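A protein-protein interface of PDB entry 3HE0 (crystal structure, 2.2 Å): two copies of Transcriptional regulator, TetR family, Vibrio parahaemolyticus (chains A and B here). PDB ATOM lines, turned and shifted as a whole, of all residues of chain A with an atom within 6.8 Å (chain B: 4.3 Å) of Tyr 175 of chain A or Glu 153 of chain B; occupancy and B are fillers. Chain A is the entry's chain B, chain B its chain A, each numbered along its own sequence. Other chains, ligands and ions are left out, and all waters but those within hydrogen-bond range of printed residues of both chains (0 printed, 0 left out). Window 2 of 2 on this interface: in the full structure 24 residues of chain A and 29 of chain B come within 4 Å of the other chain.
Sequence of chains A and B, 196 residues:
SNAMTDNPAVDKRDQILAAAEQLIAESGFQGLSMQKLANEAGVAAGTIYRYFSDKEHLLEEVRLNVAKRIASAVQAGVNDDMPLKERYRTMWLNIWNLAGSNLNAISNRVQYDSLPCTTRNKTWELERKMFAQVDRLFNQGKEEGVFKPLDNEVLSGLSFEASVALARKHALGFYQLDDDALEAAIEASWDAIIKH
Of the printed residues of chain B, Leu 166 of chain A touches Glu 153 (3.8 Å), Val 154 (3.7 Å) and Gly 157 (3.8 Å). Leu 172 of chain A touches none of the printed residues of chain B. Tyr 175 of chain A touches just these residues of chain B: Asp 151 (3.0 Å), Glu 153 (3.98 Å) and Val 154 (3.8 Å). Printed residues of chain A within 4 Å of Glu 153 of chain B: Leu 166 (3.8 Å), Lys 169 (2.8 Å) and Tyr 175 (3.98 Å). Printed residues of chain A within 4 Å of Gly 157 of chain B: Leu 166. The nearest residue of chain A that does not touch Glu 153 of chain B is Leu 177 of chain A (6.4 Å). The nearest printed residue of chain B that does not touch Lys 169 of chain A is Gly 157 of chain B (4.02 Å).
Among the printed residues, pairs that only touch across the chains: Tyr 175 of chain A with Asp 151 of chain B, Leu 166 of chain A with Val 154 of chain B, Tyr 175 of chain A with Val 154 of chain B, Leu 166 of chain A with Glu 153 of chain B, Leu 166 of chain A with Gly 157 of chain B and Tyr 175 of chain A with Glu 153 of chain B.
Of the 14 printed residues of chain A, 3 touch a printed residue of chain B. Hydrophobic or aromatic side chains of chain B that line the printed part of chain A: Val 154. Among the printed residues, Asp or Glu carboxylates within 4 Å of a Lys or Arg side-chain nitrogen of the other chain: Lys 169 of chain A with Glu 153 of chain B (2.8 Å).
The side-chain amino group (NZ) of Lys 169 of chain A lies within salt-bridge range of the side-chain carboxylate (OE1) of Glu 153 of chain B (2.8 Å).
OE2 of Glu 153 of chain B is in salt-bridge range of NH1 of Arg 128 of chain B (3.7 Å). OD2 of Asp 151 of chain B lies within hydrogen-bond range of N of Glu 153 of chain B (2.6 Å). The backbone carbonyl oxygen (O) of Lys 169 of chain A is in hydrogen-bond range of the backbone NH (N) of Phe 174 of chain A (3.0 Å). O of Lys 169 of chain A sits at hydrogen-bond distance from N of Tyr 175 of chain A, at 3.4 Å.
No position is printed for both chains. Of the 7 pairs that touch across the chains among the printed residues, none has its exchanged pair printed and touching as well.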
ATOM      1  N   TRP A  96      -5.116  29.171  13.703  1.00  0.00           N
ATOM      2  CA  TRP A  96      -3.788  29.697  13.877  1.00  0.00           C
ATOM      3  C   TRP A  96      -3.720  31.100  13.318  1.00  0.00           C
ATOM      4  O   TRP A  96      -3.195  32.016  13.949  1.00  0.00           O
ATOM      5  CB  TRP A  96      -2.796  28.778  13.168  1.00  0.00           C
ATOM      6  CG  TRP A  96      -1.415  29.299  13.147  1.00  0.00           C
ATOM      7  CD1 TRP A  96      -0.876  30.117  12.209  1.00  0.00           C
ATOM      8  CD2 TRP A  96      -0.379  29.035  14.093  1.00  0.00           C
ATOM      9  NE1 TRP A  96       0.429  30.376  12.510  1.00  0.00           N
ATOM     10  CE2 TRP A  96       0.762  29.738  13.664  1.00  0.00           C
ATOM     11  CE3 TRP A  96      -0.301  28.274  15.249  1.00  0.00           C
ATOM     12  CZ2 TRP A  96       1.967  29.723  14.361  1.00  0.00           C
ATOM     13  CZ3 TRP A  96       0.918  28.251  15.950  1.00  0.00           C
ATOM     14  CH2 TRP A  96       2.027  28.971  15.498  1.00  0.00           C
ATOM     15  N   LEU A 166      -0.696  28.167  21.048  1.00  0.00           N
ATOM     16  CA  LEU A 166       0.534  28.297  20.304  1.00  0.00           C
ATOM     17  C   LEU A 166       0.458  29.534  19.416  1.00  0.00           C
ATOM     18  O   LEU A 166       1.386  30.373  19.399  1.00  0.00           O
ATOM     19  CB  LEU A 166       0.746  27.014  19.466  1.00  0.00           C
ATOM     20  CG  LEU A 166       1.065  25.694  20.182  1.00  0.00           C
ATOM     21  CD1 LEU A 166       0.893  24.479  19.271  1.00  0.00           C
ATOM     22  CD2 LEU A 166       2.480  25.755  20.790  1.00  0.00           C
ATOM     23  N   ALA A 167      -0.665  29.689  18.713  1.00  0.00           N
ATOM     24  CA  ALA A 167      -0.845  30.841  17.848  1.00  0.00           C
ATOM     25  C   ALA A 167      -0.760  32.135  18.645  1.00  0.00           C
ATOM     26  O   ALA A 167      -0.146  33.101  18.190  1.00  0.00           O
ATOM     27  CB  ALA A 167      -2.183  30.760  17.044  1.00  0.00           C
ATOM     28  N   LYS A 169       0.888  32.842  21.539  1.00  0.00           N
ATOM     29  CA  LYS A 169       2.288  33.094  21.933  1.00  0.00           C
ATOM     30  C   LYS A 169       3.086  33.529  20.726  1.00  0.00           C
ATOM     31  O   LYS A 169       3.971  34.368  20.800  1.00  0.00           O
ATOM     32  CB  LYS A 169       2.920  31.830  22.529  1.00  0.00           C
ATOM     33  CG  LYS A 169       2.365  31.449  23.900  1.00  0.00           C
ATOM     34  CD  LYS A 169       3.257  30.449  24.680  1.00  0.00           C
ATOM     35  CE  LYS A 169       3.568  29.171  23.862  1.00  0.00           C
ATOM     36  NZ  LYS A 169       3.520  27.916  24.724  1.00  0.00           N
ATOM     37  N   HIS A 170       2.737  32.942  19.595  1.00  0.00           N
ATOM     38  CA  HIS A 170       3.371  33.274  18.343  1.00  0.00           C
ATOM     39  C   HIS A 170       3.025  34.671  17.869  1.00  0.00           C
ATOM     40  O   HIS A 170       3.905  35.395  17.429  1.00  0.00           O
ATOM     41  CB  HIS A 170       2.999  32.233  17.267  1.00  0.00           C
ATOM     42  CG  HIS A 170       3.698  32.466  15.980  1.00  0.00           C
ATOM     43  ND1 HIS A 170       3.183  33.284  14.999  1.00  0.00           N
ATOM     44  CD2 HIS A 170       4.921  32.080  15.550  1.00  0.00           C
ATOM     45  CE1 HIS A 170       4.045  33.360  13.998  1.00  0.00           C
ATOM     46  NE2 HIS A 170       5.105  32.631  14.305  1.00  0.00           N
ATOM     47  N   ALA A 171       1.751  35.060  17.941  1.00  0.00           N
ATOM     48  CA  ALA A 171       1.354  36.386  17.463  1.00  0.00           C
ATOM     49  C   ALA A 171       1.969  37.466  18.331  1.00  0.00           C
ATOM     50  O   ALA A 171       2.256  38.566  17.852  1.00  0.00           O
ATOM     51  CB  ALA A 171      -0.152  36.549  17.442  1.00  0.00           C
ATOM     52  N   LEU A 172       2.149  37.161  19.616  1.00  0.00           N
ATOM     53  CA  LEU A 172       2.672  38.141  20.571  1.00  0.00           C
ATOM     54  C   LEU A 172       4.142  38.378  20.317  1.00  0.00           C
ATOM     55  O   LEU A 172       4.707  39.317  20.829  1.00  0.00           O
ATOM     56  CB  LEU A 172       2.464  37.678  22.012  1.00  0.00           C
ATOM     57  CG  LEU A 172       1.004  37.680  22.451  1.00  0.00           C
ATOM     58  CD1 LEU A 172       0.884  37.098  23.840  1.00  0.00           C
ATOM     59  CD2 LEU A 172       0.422  39.078  22.377  1.00  0.00           C
ATOM     60  N   GLY A 173       4.762  37.513  19.522  1.00  0.00           N
ATOM     61  CA  GLY A 173       6.170  37.650  19.225  1.00  0.00           C
ATOM     62  C   GLY A 173       6.991  36.965  20.291  1.00  0.00           C
ATOM     63  O   GLY A 173       8.188  37.178  20.372  1.00  0.00           O
ATOM     64  N   PHE A 174       6.353  36.138  21.105  1.00  0.00           N
ATOM     65  CA  PHE A 174       7.037  35.488  22.208  1.00  0.00           C
ATOM     66  C   PHE A 174       7.883  34.345  21.694  1.00  0.00           C
ATOM     67  O   PHE A 174       9.093  34.311  21.897  1.00  0.00           O
ATOM     68  CB  PHE A 174       6.024  35.031  23.270  1.00  0.00           C
ATOM     69  CG  PHE A 174       5.627  36.127  24.246  1.00  0.00           C
ATOM     70  CD1 PHE A 174       5.992  37.472  24.032  1.00  0.00           C
ATOM     71  CD2 PHE A 174       4.891  35.821  25.382  1.00  0.00           C
ATOM     72  CE1 PHE A 174       5.643  38.471  24.940  1.00  0.00           C
ATOM     73  CE2 PHE A 174       4.528  36.825  26.291  1.00  0.00           C
ATOM     74  CZ  PHE A 174       4.907  38.149  26.068  1.00  0.00           C
ATOM     75  N   TYR A 175       7.249  33.433  20.987  1.00  0.00           N
ATOM     76  CA  TYR A 175       7.920  32.266  20.477  1.00  0.00           C
ATOM     77  C   TYR A 175       7.660  32.116  18.977  1.00  0.00           C
ATOM     78  O   TYR A 175       6.532  32.297  18.538  1.00  0.00           O
ATOM     79  CB  TYR A 175       7.401  31.034  21.213  1.00  0.00           C
ATOM     80  CG  TYR A 175       8.145  29.843  20.754  1.00  0.00           C
ATOM     81  CD1 TYR A 175       9.515  29.740  21.003  1.00  0.00           C
ATOM     82  CD2 TYR A 175       7.532  28.868  19.988  1.00  0.00           C
ATOM     83  CE1 TYR A 175      10.261  28.655  20.545  1.00  0.00           C
ATOM     84  CE2 TYR A 175       8.264  27.770  19.521  1.00  0.00           C
ATOM     85  CZ  TYR A 175       9.639  27.676  19.805  1.00  0.00           C
ATOM     86  OH  TYR A 175      10.395  26.618  19.349  1.00  0.00           O
ATOM     87  N   GLN A 176       8.680  31.751  18.203  1.00  0.00           N
ATOM     88  CA  GLN A 176       8.548  31.569  16.736  1.00  0.00           C
ATOM     89  C   GLN A 176       8.617  30.075  16.375  1.00  0.00           C
ATOM     90  O   GLN A 176       9.514  29.369  16.818  1.00  0.00           O
ATOM     91  CB  GLN A 176       9.644  32.364  15.985  1.00  0.00           C
ATOM     92  N   LEU A 177       7.644  29.592  15.606  1.00  0.00           N
ATOM     93  CA  LEU A 177       7.625  28.213  15.125  1.00  0.00           C
ATOM     94  C   LEU A 177       7.950  28.187  13.649  1.00  0.00           C
ATOM     95  O   LEU A 177       7.114  28.606  12.859  1.00  0.00           O
ATOM     96  CB  LEU A 177       6.226  27.615  15.248  1.00  0.00           C
ATOM     97  CG  LEU A 177       5.830  26.881  16.515  1.00  0.00           C
ATOM     98  CD1 LEU A 177       5.411  27.862  17.636  1.00  0.00           C
ATOM     99  CD2 LEU A 177       4.671  25.927  16.208  1.00  0.00           C
ATOM    100  N   ASP A 178       9.091  27.647  13.237  1.00  0.00           N
ATOM    101  CA  ASP A 178       9.292  27.443  11.801  1.00  0.00           C
ATOM    102  C   ASP A 178       8.305  26.418  11.210  1.00  0.00           C
ATOM    103  O   ASP A 178       7.509  25.779  11.939  1.00  0.00           O
ATOM    104  CB  ASP A 178      10.751  27.128  11.470  1.00  0.00           C
ATOM    105  CG  ASP A 178      11.134  25.693  11.715  1.00  0.00           C
ATOM    106  OD1 ASP A 178      10.289  24.837  12.088  1.00  0.00           O
ATOM    107  OD2 ASP A 178      12.337  25.412  11.510  1.00  0.00           O
ATOM    108  N   ALA A 181       8.292  22.741  12.381  1.00  0.00           N
ATOM    109  CA  ALA A 181       7.728  22.768  13.738  1.00  0.00           C
ATOM    110  C   ALA A 181       6.210  22.923  13.754  1.00  0.00           C
ATOM    111  O   ALA A 181       5.512  22.250  14.501  1.00  0.00           O
ATOM    112  CB  ALA A 181       8.428  23.885  14.598  1.00  0.00           C
ATOM    113  N   ARG B 128       9.185  32.959  32.304  1.00  0.00           N
ATOM    114  CA  ARG B 128       9.597  31.620  31.875  1.00  0.00           C
ATOM    115  C   ARG B 128      10.481  30.975  32.940  1.00  0.00           C
ATOM    116  O   ARG B 128      10.210  29.861  33.385  1.00  0.00           O
ATOM    117  CB  ARG B 128      10.311  31.660  30.528  1.00  0.00           C
ATOM    118  CG  ARG B 128       9.995  30.474  29.637  1.00  0.00           C
ATOM    119  CD  ARG B 128      10.975  29.336  29.851  1.00  0.00           C
ATOM    120  NE  ARG B 128      10.636  28.124  29.096  1.00  0.00           N
ATOM    121  CZ  ARG B 128      10.932  27.900  27.813  1.00  0.00           C
ATOM    122  NH1 ARG B 128      10.594  26.743  27.257  1.00  0.00           N
ATOM    123  NH2 ARG B 128      11.558  28.811  27.075  1.00  0.00           N
ATOM    124  N   ASP B 151      10.370  21.986  20.846  1.00  0.00           N
ATOM    125  CA  ASP B 151      10.666  22.979  21.883  1.00  0.00           C
ATOM    126  C   ASP B 151       9.676  22.832  23.028  1.00  0.00           C
ATOM    127  O   ASP B 151       8.483  22.520  22.791  1.00  0.00           O
ATOM    128  CB  ASP B 151      10.548  24.405  21.319  1.00  0.00           C
ATOM    129  CG  ASP B 151      10.955  25.494  22.345  1.00  0.00           C
ATOM    130  OD1 ASP B 151      12.148  25.881  22.353  1.00  0.00           O
ATOM    131  OD2 ASP B 151      10.099  25.942  23.164  1.00  0.00           O
ATOM    132  N   ASN B 152      10.151  23.101  24.248  1.00  0.00           N
ATOM    133  CA  ASN B 152       9.308  23.031  25.438  1.00  0.00           C
ATOM    134  C   ASN B 152       8.083  23.953  25.359  1.00  0.00           C
ATOM    135  O   ASN B 152       7.050  23.653  25.935  1.00  0.00           O
ATOM    136  CB  ASN B 152      10.116  23.341  26.716  1.00  0.00           C
ATOM    137  CG  ASN B 152      11.152  22.269  27.042  1.00  0.00           C
ATOM    138  OD1 ASN B 152      11.283  21.279  26.338  1.00  0.00           O
ATOM    139  ND2 ASN B 152      11.893  22.473  28.126  1.00  0.00           N
ATOM    140  N   GLU B 153       8.191  25.056  24.631  1.00  0.00           N
ATOM    141  CA  GLU B 153       7.051  25.947  24.401  1.00  0.00           C
ATOM    142  C   GLU B 153       5.946  25.276  23.584  1.00  0.00           C
ATOM    143  O   GLU B 153       4.750  25.519  23.832  1.00  0.00           O
ATOM    144  CB  GLU B 153       7.492  27.238  23.688  1.00  0.00           C
ATOM    145  CG  GLU B 153       8.188  28.252  24.617  1.00  0.00           C
ATOM    146  CD  GLU B 153       7.264  28.776  25.729  1.00  0.00           C
ATOM    147  OE1 GLU B 153       6.039  28.925  25.475  1.00  0.00           O
ATOM    148  OE2 GLU B 153       7.761  29.039  26.866  1.00  0.00           O
ATOM    149  N   VAL B 154       6.351  24.430  22.630  1.00  0.00           N
ATOM    150  CA  VAL B 154       5.395  23.700  21.789  1.00  0.00           C
ATOM    151  C   VAL B 154       4.792  22.552  22.620  1.00  0.00           C
ATOM    152  O   VAL B 154       3.584  22.369  22.675  1.00  0.00           O
ATOM    153  CB  VAL B 154       6.064  23.198  20.516  1.00  0.00           C
ATOM    154  CG1 VAL B 154       5.107  22.310  19.661  1.00  0.00           C
ATOM    155  CG2 VAL B 154       6.592  24.379  19.704  1.00  0.00           C
ATOM    156  N   LEU B 155       5.637  21.803  23.318  1.00  0.00           N
ATOM    157  CA  LEU B 155       5.149  20.736  24.174  1.00  0.00           C
ATOM    158  C   LEU B 155       4.138  21.302  25.196  1.00  0.00           C
ATOM    159  O   LEU B 155       3.075  20.727  25.428  1.00  0.00           O
ATOM    160  CB  LEU B 155       6.321  20.045  24.874  1.00  0.00           C
ATOM    161  CG  LEU B 155       7.299  19.294  23.957  1.00  0.00           C
ATOM    162  CD1 LEU B 155       8.468  18.735  24.791  1.00  0.00           C
ATOM    163  CD2 LEU B 155       6.582  18.193  23.150  1.00  0.00           C
ATOM    164  N   SER B 156       4.444  22.469  25.764  1.00  0.00           N
ATOM    165  CA  SER B 156       3.534  23.075  26.735  1.00  0.00           C
ATOM    166  C   SER B 156       2.213  23.462  26.069  1.00  0.00           C
ATOM    167  O   SER B 156       1.139  23.155  26.596  1.00  0.00           O
ATOM    168  CB  SER B 156       4.163  24.282  27.426  1.00  0.00           C
ATOM    169  OG  SER B 156       3.306  24.770  28.486  1.00  0.00           O
ATOM    170  N   GLY B 157       2.303  24.086  24.897  1.00  0.00           N
ATOM    171  CA  GLY B 157       1.112  24.475  24.142  1.00  0.00           C
ATOM    172  C   GLY B 157       0.215  23.295  23.791  1.00  0.00           C
ATOM    173  O   GLY B 157      -0.978  23.448  23.731  1.00  0.00           O
